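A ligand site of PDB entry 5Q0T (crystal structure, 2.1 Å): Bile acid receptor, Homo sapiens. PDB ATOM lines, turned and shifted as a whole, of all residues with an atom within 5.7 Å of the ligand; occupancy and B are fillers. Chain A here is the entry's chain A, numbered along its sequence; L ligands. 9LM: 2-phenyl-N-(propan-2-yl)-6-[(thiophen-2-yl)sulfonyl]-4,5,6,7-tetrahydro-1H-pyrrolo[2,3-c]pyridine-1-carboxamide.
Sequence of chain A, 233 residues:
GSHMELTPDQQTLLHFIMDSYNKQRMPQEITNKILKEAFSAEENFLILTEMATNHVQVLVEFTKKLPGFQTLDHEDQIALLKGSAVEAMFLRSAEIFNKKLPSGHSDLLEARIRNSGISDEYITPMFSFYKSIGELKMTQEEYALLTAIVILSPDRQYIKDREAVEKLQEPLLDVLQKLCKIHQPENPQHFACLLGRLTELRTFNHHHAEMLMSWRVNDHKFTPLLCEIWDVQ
N26 of the ligand is in hydrogen-bond range of OG of Ser 93 (2.8 Å).
An oxygen (O25) of the ligand sits at hydrogen-bond distance from the backbone NH of Ala 52 (3.4 Å).
The side-chain sulfur (SD) of Met 89 sits close to a nitrogen (N26) of the ligand (3.8 Å).
OG of Ser 93 sits at hydrogen-bond distance from O of Met 89.
The side-chain hydroxyl (OG1) of Thr 49 lies within hydrogen-bond range of the backbone carbonyl oxygen (O) of Phe 45, at 3.0 Å.
The side-chain sulfur (SD) of Met 126 sits close to the side-chain hydroxyl (OH) of Tyr 130 (3.4 Å).
The backbone NH (N) of Met 89 lies within hydrogen-bond range of a ring nitrogen (NE2) of His 55, 3.3 Å away.
The backbone carbonyl oxygen (O) of Ile 96 sits at hydrogen-bond distance from the backbone NH (N) of Leu 101, 3.5 Å away.
Residues that only touch the ligand: Thr 49 (3.0 Å), His 208 (3.1 Å), Tyr 130 (3.2 Å), Trp 230 (3.3 Å), Met 51 (3.4 Å), Phe 45 (3.4 Å), Ile 113 (3.6 Å), Leu 109 (3.6 Å), Phe 222 (3.6 Å), Ile 96 (3.6 Å), Leu 48 (3.6 Å), Arg 92 (3.7 Å) and Met 126 (3.8 Å).
Hydrophobic or aromatic side chains within 4 Å of the ligand: Phe 45, Leu 48, Met 51, Ala 52, Met 89, Ile 96, Leu 109, Ile 113, Met 126, Tyr 130, His 208, Phe 222 and Trp 230.
Within 4 Å of the ligand: Phe 45, Leu 48, Thr 49, Met 51, Ala 52, Met 89, Arg 92, Ser 93, Ile 96, Leu 109, Ile 113, Met 126, Tyr 130, His 208, Phe 222 and Trp 230.
The nearest printed residue that does not touch the ligand is Ile 118 (4.03 Å).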
ATOM      1  N   PHE A  45       7.968   6.665  23.764  1.00  0.00           N
ATOM      2  CA  PHE A  45       7.377   5.347  23.503  1.00  0.00           C
ATOM      3  C   PHE A  45       5.987   5.282  24.136  1.00  0.00           C
ATOM      4  O   PHE A  45       5.085   4.674  23.559  1.00  0.00           O
ATOM      5  CB  PHE A  45       8.246   4.195  24.020  1.00  0.00           C
ATOM      6  CG  PHE A  45       7.857   2.841  23.486  1.00  0.00           C
ATOM      7  CD1 PHE A  45       6.941   2.032  24.172  1.00  0.00           C
ATOM      8  CD2 PHE A  45       8.386   2.361  22.298  1.00  0.00           C
ATOM      9  CE1 PHE A  45       6.565   0.791  23.662  1.00  0.00           C
ATOM     10  CE2 PHE A  45       8.025   1.112  21.791  1.00  0.00           C
ATOM     11  CZ  PHE A  45       7.125   0.336  22.482  1.00  0.00           C
ATOM     12  N   LEU A  48       3.429   7.205  21.815  1.00  0.00           N
ATOM     13  CA  LEU A  48       3.009   6.382  20.673  1.00  0.00           C
ATOM     14  C   LEU A  48       2.006   5.301  21.119  1.00  0.00           C
ATOM     15  O   LEU A  48       1.045   5.030  20.395  1.00  0.00           O
ATOM     16  CB  LEU A  48       4.205   5.750  19.959  1.00  0.00           C
ATOM     17  CG  LEU A  48       5.114   6.671  19.125  1.00  0.00           C
ATOM     18  CD1 LEU A  48       6.337   5.918  18.610  1.00  0.00           C
ATOM     19  CD2 LEU A  48       4.360   7.294  17.964  1.00  0.00           C
ATOM     20  N   THR A  49       2.210   4.733  22.320  1.00  0.00           N
ATOM     21  CA  THR A  49       1.313   3.743  22.937  1.00  0.00           C
ATOM     22  C   THR A  49      -0.081   4.353  23.134  1.00  0.00           C
ATOM     23  O   THR A  49      -1.072   3.720  22.759  1.00  0.00           O
ATOM     24  CB  THR A  49       1.985   3.163  24.204  1.00  0.00           C
ATOM     25  OG1 THR A  49       3.114   2.390  23.785  1.00  0.00           O
ATOM     26  CG2 THR A  49       1.049   2.260  25.020  1.00  0.00           C
ATOM     27  N   MET A  51      -1.328   7.127  21.548  1.00  0.00           N
ATOM     28  CA  MET A  51      -1.862   7.423  20.215  1.00  0.00           C
ATOM     29  C   MET A  51      -2.398   6.177  19.494  1.00  0.00           C
ATOM     30  O   MET A  51      -3.496   6.230  18.952  1.00  0.00           O
ATOM     31  CB  MET A  51      -0.814   8.141  19.349  1.00  0.00           C
ATOM     32  CG  MET A  51      -0.463   9.524  19.848  1.00  0.00           C
ATOM     33  SD  MET A  51       0.806  10.266  18.815  1.00  0.00           S
ATOM     34  CE  MET A  51      -0.203  11.042  17.567  1.00  0.00           C
ATOM     35  N   ALA A  52      -1.643   5.064  19.536  1.00  0.00           N
ATOM     36  CA  ALA A  52      -2.040   3.805  18.878  1.00  0.00           C
ATOM     37  C   ALA A  52      -3.289   3.191  19.516  1.00  0.00           C
ATOM     38  O   ALA A  52      -4.129   2.644  18.806  1.00  0.00           O
ATOM     39  CB  ALA A  52      -0.890   2.811  18.875  1.00  0.00           C
ATOM     40  N   HIS A  55      -6.315   5.273  18.453  1.00  0.00           N
ATOM     41  CA  HIS A  55      -6.605   4.878  17.069  1.00  0.00           C
ATOM     42  C   HIS A  55      -7.463   3.599  16.970  1.00  0.00           C
ATOM     43  O   HIS A  55      -8.387   3.575  16.159  1.00  0.00           O
ATOM     44  CB  HIS A  55      -5.319   4.774  16.218  1.00  0.00           C
ATOM     45  CG  HIS A  55      -5.584   4.094  14.908  1.00  0.00           C
ATOM     46  ND1 HIS A  55      -6.280   4.732  13.899  1.00  0.00           N
ATOM     47  CD2 HIS A  55      -5.338   2.820  14.531  1.00  0.00           C
ATOM     48  CE1 HIS A  55      -6.390   3.833  12.925  1.00  0.00           C
ATOM     49  NE2 HIS A  55      -5.853   2.663  13.273  1.00  0.00           N
ATOM     50  N   ALA A  88      -4.379  -0.145   9.090  1.00  0.00           N
ATOM     51  CA  ALA A  88      -5.220   1.038   9.320  1.00  0.00           C
ATOM     52  C   ALA A  88      -4.435   2.088  10.108  1.00  0.00           C
ATOM     53  O   ALA A  88      -4.541   3.268   9.798  1.00  0.00           O
ATOM     54  CB  ALA A  88      -6.485   0.652  10.071  1.00  0.00           C
ATOM     55  N   MET A  89      -3.614   1.647  11.091  1.00  0.00           N
ATOM     56  CA  MET A  89      -2.756   2.543  11.878  1.00  0.00           C
ATOM     57  C   MET A  89      -1.746   3.290  10.978  1.00  0.00           C
ATOM     58  O   MET A  89      -1.618   4.496  11.097  1.00  0.00           O
ATOM     59  CB  MET A  89      -2.085   1.772  13.052  1.00  0.00           C
ATOM     60  CG  MET A  89      -1.217   2.633  13.971  1.00  0.00           C
ATOM     61  SD  MET A  89       0.416   3.090  13.269  1.00  0.00           S
ATOM     62  CE  MET A  89       1.245   1.504  13.315  1.00  0.00           C
ATOM     63  N   PHE A  90      -1.034   2.584  10.095  1.00  0.00           N
ATOM     64  CA  PHE A  90      -0.052   3.200   9.199  1.00  0.00           C
ATOM     65  C   PHE A  90      -0.672   4.178   8.176  1.00  0.00           C
ATOM     66  O   PHE A  90      -0.047   5.181   7.821  1.00  0.00           O
ATOM     67  CB  PHE A  90       0.810   2.152   8.484  1.00  0.00           C
ATOM     68  CG  PHE A  90       1.919   1.543   9.332  1.00  0.00           C
ATOM     69  CD1 PHE A  90       3.106   2.235   9.554  1.00  0.00           C
ATOM     70  CD2 PHE A  90       1.780   0.271   9.863  1.00  0.00           C
ATOM     71  CE1 PHE A  90       4.117   1.680  10.333  1.00  0.00           C
ATOM     72  CE2 PHE A  90       2.804  -0.300  10.634  1.00  0.00           C
ATOM     73  CZ  PHE A  90       3.964   0.416  10.861  1.00  0.00           C
ATOM     74  N   ARG A  92      -3.626   5.911   8.639  1.00  0.00           N
ATOM     75  CA  ARG A  92      -4.078   7.046   9.428  1.00  0.00           C
ATOM     76  C   ARG A  92      -2.853   7.919   9.837  1.00  0.00           C
ATOM     77  O   ARG A  92      -2.954   9.142   9.790  1.00  0.00           O
ATOM     78  CB  ARG A  92      -4.889   6.549  10.643  1.00  0.00           C
ATOM     79  CG  ARG A  92      -5.390   7.625  11.615  1.00  0.00           C
ATOM     80  CD  ARG A  92      -6.259   8.693  11.009  1.00  0.00           C
ATOM     81  NE  ARG A  92      -6.466   9.778  11.968  1.00  0.00           N
ATOM     82  CZ  ARG A  92      -7.266  10.816  11.794  1.00  0.00           C
ATOM     83  NH1 ARG A  92      -7.982  10.935  10.672  1.00  0.00           N
ATOM     84  NH2 ARG A  92      -7.390  11.745  12.733  1.00  0.00           N
ATOM     85  N   SER A  93      -1.711   7.273  10.191  1.00  0.00           N
ATOM     86  CA  SER A  93      -0.432   7.910  10.550  1.00  0.00           C
ATOM     87  C   SER A  93       0.056   8.814   9.389  1.00  0.00           C
ATOM     88  O   SER A  93       0.437   9.962   9.619  1.00  0.00           O
ATOM     89  CB  SER A  93       0.624   6.841  10.849  1.00  0.00           C
ATOM     90  OG  SER A  93       0.379   6.149  12.054  1.00  0.00           O
ATOM     91  N   ALA A  94      -0.018   8.289   8.147  1.00  0.00           N
ATOM     92  CA  ALA A  94       0.304   8.971   6.895  1.00  0.00           C
ATOM     93  C   ALA A  94      -0.603  10.167   6.735  1.00  0.00           C
ATOM     94  O   ALA A  94      -0.107  11.239   6.418  1.00  0.00           O
ATOM     95  CB  ALA A  94       0.114   8.031   5.711  1.00  0.00           C
ATOM     96  N   ILE A  96      -2.381  11.940   9.203  1.00  0.00           N
ATOM     97  CA  ILE A  96      -2.000  12.894  10.244  1.00  0.00           C
ATOM     98  C   ILE A  96      -0.707  13.671   9.881  1.00  0.00           C
ATOM     99  O   ILE A  96      -0.649  14.880  10.071  1.00  0.00           O
ATOM    100  CB  ILE A  96      -1.879  12.206  11.641  1.00  0.00           C
ATOM    101  CG1 ILE A  96      -3.238  11.694  12.126  1.00  0.00           C
ATOM    102  CG2 ILE A  96      -1.241  13.129  12.693  1.00  0.00           C
ATOM    103  CD1 ILE A  96      -3.152  10.502  13.043  1.00  0.00           C
ATOM    104  N   PHE A  97       0.316  12.958   9.352  1.00  0.00           N
ATOM    105  CA  PHE A  97       1.623  13.491   8.956  1.00  0.00           C
ATOM    106  C   PHE A  97       1.542  14.496   7.818  1.00  0.00           C
ATOM    107  O   PHE A  97       2.241  15.514   7.855  1.00  0.00           O
ATOM    108  CB  PHE A  97       2.630  12.353   8.628  1.00  0.00           C
ATOM    109  CG  PHE A  97       3.964  12.790   8.072  1.00  0.00           C
ATOM    110  CD1 PHE A  97       5.034  13.052   8.919  1.00  0.00           C
ATOM    111  CD2 PHE A  97       4.161  12.933   6.692  1.00  0.00           C
ATOM    112  CE1 PHE A  97       6.277  13.441   8.406  1.00  0.00           C
ATOM    113  CE2 PHE A  97       5.412  13.326   6.182  1.00  0.00           C
ATOM    114  CZ  PHE A  97       6.463  13.568   7.041  1.00  0.00           C
ATOM    115  N   LEU A 101      -1.745  17.848  11.519  1.00  0.00           N
ATOM    116  CA  LEU A 101      -0.833  18.519  12.464  1.00  0.00           C
ATOM    117  C   LEU A 101      -0.201  19.828  11.990  1.00  0.00           C
ATOM    118  O   LEU A 101       0.273  19.870  10.854  1.00  0.00           O
ATOM    119  CB  LEU A 101       0.282  17.574  12.889  1.00  0.00           C
ATOM    120  CG  LEU A 101       0.000  16.644  14.031  1.00  0.00           C
ATOM    121  CD1 LEU A 101       1.091  15.667  14.112  1.00  0.00           C
ATOM    122  CD2 LEU A 101      -0.093  17.376  15.364  1.00  0.00           C
ATOM    123  N   LEU A 109       6.461  15.995  16.917  1.00  0.00           N
ATOM    124  CA  LEU A 109       5.953  14.616  16.818  1.00  0.00           C
ATOM    125  C   LEU A 109       6.974  13.700  16.132  1.00  0.00           C
ATOM    126  O   LEU A 109       7.281  12.637  16.671  1.00  0.00           O
ATOM    127  CB  LEU A 109       4.592  14.535  16.123  1.00  0.00           C
ATOM    128  CG  LEU A 109       3.902  13.147  16.058  1.00  0.00           C
ATOM    129  CD1 LEU A 109       3.896  12.437  17.409  1.00  0.00           C
ATOM    130  CD2 LEU A 109       2.488  13.280  15.628  1.00  0.00           C
ATOM    131  N   ILE A 113       8.787  10.399  17.405  1.00  0.00           N
ATOM    132  CA  ILE A 113       8.700   9.128  16.673  1.00  0.00           C
ATOM    133  C   ILE A 113      10.131   8.611  16.389  1.00  0.00           C
ATOM    134  O   ILE A 113      10.367   7.412  16.514  1.00  0.00           O
ATOM    135  CB  ILE A 113       7.810   9.222  15.369  1.00  0.00           C
ATOM    136  CG1 ILE A 113       6.334   9.578  15.706  1.00  0.00           C
ATOM    137  CG2 ILE A 113       7.858   7.922  14.535  1.00  0.00           C
ATOM    138  CD1 ILE A 113       5.500  10.077  14.490  1.00  0.00           C
ATOM    139  N   ILE A 118      12.833   2.927  18.853  1.00  0.00           N
ATOM    140  CA  ILE A 118      12.510   2.054  17.721  1.00  0.00           C
ATOM    141  C   ILE A 118      13.654   2.157  16.710  1.00  0.00           C
ATOM    142  O   ILE A 118      14.206   3.238  16.504  1.00  0.00           O
ATOM    143  CB  ILE A 118      11.111   2.412  17.116  1.00  0.00           C
ATOM    144  CG1 ILE A 118       9.966   2.176  18.154  1.00  0.00           C
ATOM    145  CG2 ILE A 118      10.849   1.611  15.814  1.00  0.00           C
ATOM    146  CD1 ILE A 118       8.552   2.771  17.786  1.00  0.00           C
ATOM    147  N   ILE A 123      11.810   2.763  11.163  1.00  0.00           N
ATOM    148  CA  ILE A 123      11.458   4.183  11.133  1.00  0.00           C
ATOM    149  C   ILE A 123      11.642   4.762   9.736  1.00  0.00           C
ATOM    150  O   ILE A 123      10.807   5.543   9.297  1.00  0.00           O
ATOM    151  CB  ILE A 123      12.198   5.005  12.245  1.00  0.00           C
ATOM    152  CG1 ILE A 123      11.735   4.599  13.667  1.00  0.00           C
ATOM    153  CG2 ILE A 123      12.110   6.533  12.042  1.00  0.00           C
ATOM    154  CD1 ILE A 123      10.242   4.900  14.054  1.00  0.00           C
ATOM    155  N   MET A 126       8.834   3.775   7.200  1.00  0.00           N
ATOM    156  CA  MET A 126       7.634   4.390   7.778  1.00  0.00           C
ATOM    157  C   MET A 126       7.438   5.820   7.251  1.00  0.00           C
ATOM    158  O   MET A 126       6.367   6.133   6.737  1.00  0.00           O
ATOM    159  CB  MET A 126       7.763   4.403   9.306  1.00  0.00           C
ATOM    160  CG  MET A 126       6.464   4.515  10.041  1.00  0.00           C
ATOM    161  SD  MET A 126       6.659   4.589  11.840  1.00  0.00           S
ATOM    162  CE  MET A 126       7.359   2.942  12.166  1.00  0.00           C
ATOM    163  N   TYR A 130       4.807   7.575   4.478  1.00  0.00           N
ATOM    164  CA  TYR A 130       4.070   8.830   4.660  1.00  0.00           C
ATOM    165  C   TYR A 130       4.382   9.771   3.492  1.00  0.00           C
ATOM    166  O   TYR A 130       3.464  10.302   2.889  1.00  0.00           O
ATOM    167  CB  TYR A 130       4.423   9.569   5.974  1.00  0.00           C
ATOM    168  CG  TYR A 130       4.345   8.789   7.271  1.00  0.00           C
ATOM    169  CD1 TYR A 130       3.500   7.698   7.406  1.00  0.00           C
ATOM    170  CD2 TYR A 130       5.079   9.181   8.381  1.00  0.00           C
ATOM    171  CE1 TYR A 130       3.446   6.964   8.592  1.00  0.00           C
ATOM    172  CE2 TYR A 130       5.034   8.468   9.575  1.00  0.00           C
ATOM    173  CZ  TYR A 130       4.201   7.362   9.672  1.00  0.00           C
ATOM    174  OH  TYR A 130       4.138   6.656  10.847  1.00  0.00           O
ATOM    175  N   HIS A 208       6.035  -4.654  11.325  1.00  0.00           N
ATOM    176  CA  HIS A 208       5.442  -4.533  12.662  1.00  0.00           C
ATOM    177  C   HIS A 208       5.706  -5.743  13.562  1.00  0.00           C
ATOM    178  O   HIS A 208       6.046  -5.551  14.728  1.00  0.00           O
ATOM    179  CB  HIS A 208       3.939  -4.214  12.586  1.00  0.00           C
ATOM    180  CG  HIS A 208       3.369  -3.715  13.872  1.00  0.00           C
ATOM    181  ND1 HIS A 208       3.431  -2.383  14.231  1.00  0.00           N
ATOM    182  CD2 HIS A 208       2.736  -4.395  14.861  1.00  0.00           C
ATOM    183  CE1 HIS A 208       2.843  -2.297  15.409  1.00  0.00           C
ATOM    184  NE2 HIS A 208       2.423  -3.480  15.829  1.00  0.00           N
ATOM    185  N   MET A 211       9.148  -5.702  14.561  1.00  0.00           N
ATOM    186  CA  MET A 211       9.355  -4.579  15.483  1.00  0.00           C
ATOM    187  C   MET A 211       9.173  -5.022  16.953  1.00  0.00           C
ATOM    188  O   MET A 211       9.928  -4.584  17.822  1.00  0.00           O
ATOM    189  CB  MET A 211       8.427  -3.399  15.145  1.00  0.00           C
ATOM    190  CG  MET A 211       9.163  -2.233  14.531  1.00  0.00           C
ATOM    191  SD  MET A 211       8.259  -0.655  14.444  1.00  0.00           S
ATOM    192  CE  MET A 211       7.408  -0.839  12.877  1.00  0.00           C
ATOM    193  N   PHE A 222       2.602  -3.398  26.432  1.00  0.00           N
ATOM    194  CA  PHE A 222       1.645  -2.479  25.823  1.00  0.00           C
ATOM    195  C   PHE A 222       0.268  -2.537  26.475  1.00  0.00           C
ATOM    196  O   PHE A 222       0.014  -3.383  27.343  1.00  0.00           O
ATOM    197  CB  PHE A 222       1.502  -2.805  24.327  1.00  0.00           C
ATOM    198  CG  PHE A 222       2.776  -2.812  23.519  1.00  0.00           C
ATOM    199  CD1 PHE A 222       3.586  -3.943  23.459  1.00  0.00           C
ATOM    200  CD2 PHE A 222       3.146  -1.694  22.771  1.00  0.00           C
ATOM    201  CE1 PHE A 222       4.754  -3.949  22.695  1.00  0.00           C
ATOM    202  CE2 PHE A 222       4.303  -1.714  21.992  1.00  0.00           C
ATOM    203  CZ  PHE A 222       5.106  -2.835  21.963  1.00  0.00           C
ATOM    204  N   LEU A 226      -4.075  -3.000  22.503  1.00  0.00           N
ATOM    205  CA  LEU A 226      -2.981  -3.276  21.580  1.00  0.00           C
ATOM    206  C   LEU A 226      -2.565  -4.740  21.604  1.00  0.00           C
ATOM    207  O   LEU A 226      -2.503  -5.336  20.531  1.00  0.00           O
ATOM    208  CB  LEU A 226      -1.773  -2.353  21.828  1.00  0.00           C
ATOM    209  CG  LEU A 226      -1.997  -0.854  21.607  1.00  0.00           C
ATOM    210  CD1 LEU A 226      -0.699  -0.094  21.773  1.00  0.00           C
ATOM    211  CD2 LEU A 226      -2.600  -0.554  20.230  1.00  0.00           C
ATOM    212  N   TRP A 230      -3.073  -7.082  18.313  1.00  0.00           N
ATOM    213  CA  TRP A 230      -1.834  -7.479  17.626  1.00  0.00           C
ATOM    214  C   TRP A 230      -1.452  -8.949  17.813  1.00  0.00           C
ATOM    215  O   TRP A 230      -0.586  -9.437  17.085  1.00  0.00           O
ATOM    216  CB  TRP A 230      -0.656  -6.603  18.081  1.00  0.00           C
ATOM    217  CG  TRP A 230      -0.744  -5.156  17.729  1.00  0.00           C
ATOM    218  CD1 TRP A 230      -1.499  -4.570  16.749  1.00  0.00           C
ATOM    219  CD2 TRP A 230       0.044  -4.104  18.289  1.00  0.00           C
ATOM    220  NE1 TRP A 230      -1.275  -3.217  16.721  1.00  0.00           N
ATOM    221  CE2 TRP A 230      -0.318  -2.902  17.646  1.00  0.00           C
ATOM    222  CE3 TRP A 230       1.005  -4.057  19.316  1.00  0.00           C
ATOM    223  CZ2 TRP A 230       0.241  -1.674  17.981  1.00  0.00           C
ATOM    224  CZ3 TRP A 230       1.558  -2.824  19.658  1.00  0.00           C
ATOM    225  CH2 TRP A 230       1.181  -1.654  18.979  1.00  0.00           C
HETATM  226  C4  9LM L   1       2.750   6.999  14.557  1.00  0.00           C
HETATM  227  C7  9LM L   1       4.245   2.853  15.171  1.00  0.00           C
HETATM  228  C8  9LM L   1       5.055   4.148  15.220  1.00  0.00           C
HETATM  229  C10 9LM L   1       2.275   8.297  14.047  1.00  0.00           C
HETATM  230  C13 9LM L   1       1.423  10.754  13.038  1.00  0.00           C
HETATM  231  C15 9LM L   1       2.684   8.735  12.791  1.00  0.00           C
HETATM  232  C20 9LM L   1       2.451   1.481  19.652  1.00  0.00           C
HETATM  233  C21 9LM L   1       3.063   1.611  20.918  1.00  0.00           C
HETATM  234  C22 9LM L   1       4.399   1.687  20.881  1.00  0.00           C
HETATM  235  C24 9LM L   1       0.537   6.198  15.716  1.00  0.00           C
HETATM  236  C28 9LM L   1      -2.025   7.971  15.695  1.00  0.00           C
HETATM  237  C27 9LM L   1      -1.782   6.643  15.006  1.00  0.00           C
HETATM  238  C29 9LM L   1      -2.553   6.536  13.712  1.00  0.00           C
HETATM  239  N26 9LM L   1      -0.347   6.479  14.742  1.00  0.00           N
HETATM  240  O25 9LM L   1       0.257   6.053  16.902  1.00  0.00           O
HETATM  241  N5  9LM L   1       1.917   6.069  15.315  1.00  0.00           N
HETATM  242  C1  9LM L   1       2.703   4.958  15.610  1.00  0.00           C
HETATM  243  C9  9LM L   1       2.264   3.758  16.370  1.00  0.00           C
HETATM  244  N6  9LM L   1       3.370   2.779  16.364  1.00  0.00           N
HETATM  245  C2  9LM L   1       3.956   5.166  15.078  1.00  0.00           C
HETATM  246  C3  9LM L   1       3.972   6.423  14.429  1.00  0.00           C
HETATM  247  C11 9LM L   1       1.427   9.122  14.788  1.00  0.00           C
HETATM  248  C12 9LM L   1       1.006  10.337  14.289  1.00  0.00           C
HETATM  249  C14 9LM L   1       2.261   9.957  12.286  1.00  0.00           C
HETATM  250  S16 9LM L   1       3.065   1.314  16.985  1.00  0.00           S
HETATM  251  O17 9LM L   1       1.661   1.089  16.835  1.00  0.00           O
HETATM  252  O18 9LM L   1       4.002   0.399  16.403  1.00  0.00           O
HETATM  253  C19 9LM L   1       3.407   1.456  18.673  1.00  0.00           C
HETATM  254  S23 9LM L   1       4.997   1.609  19.290  1.00  0.00           S
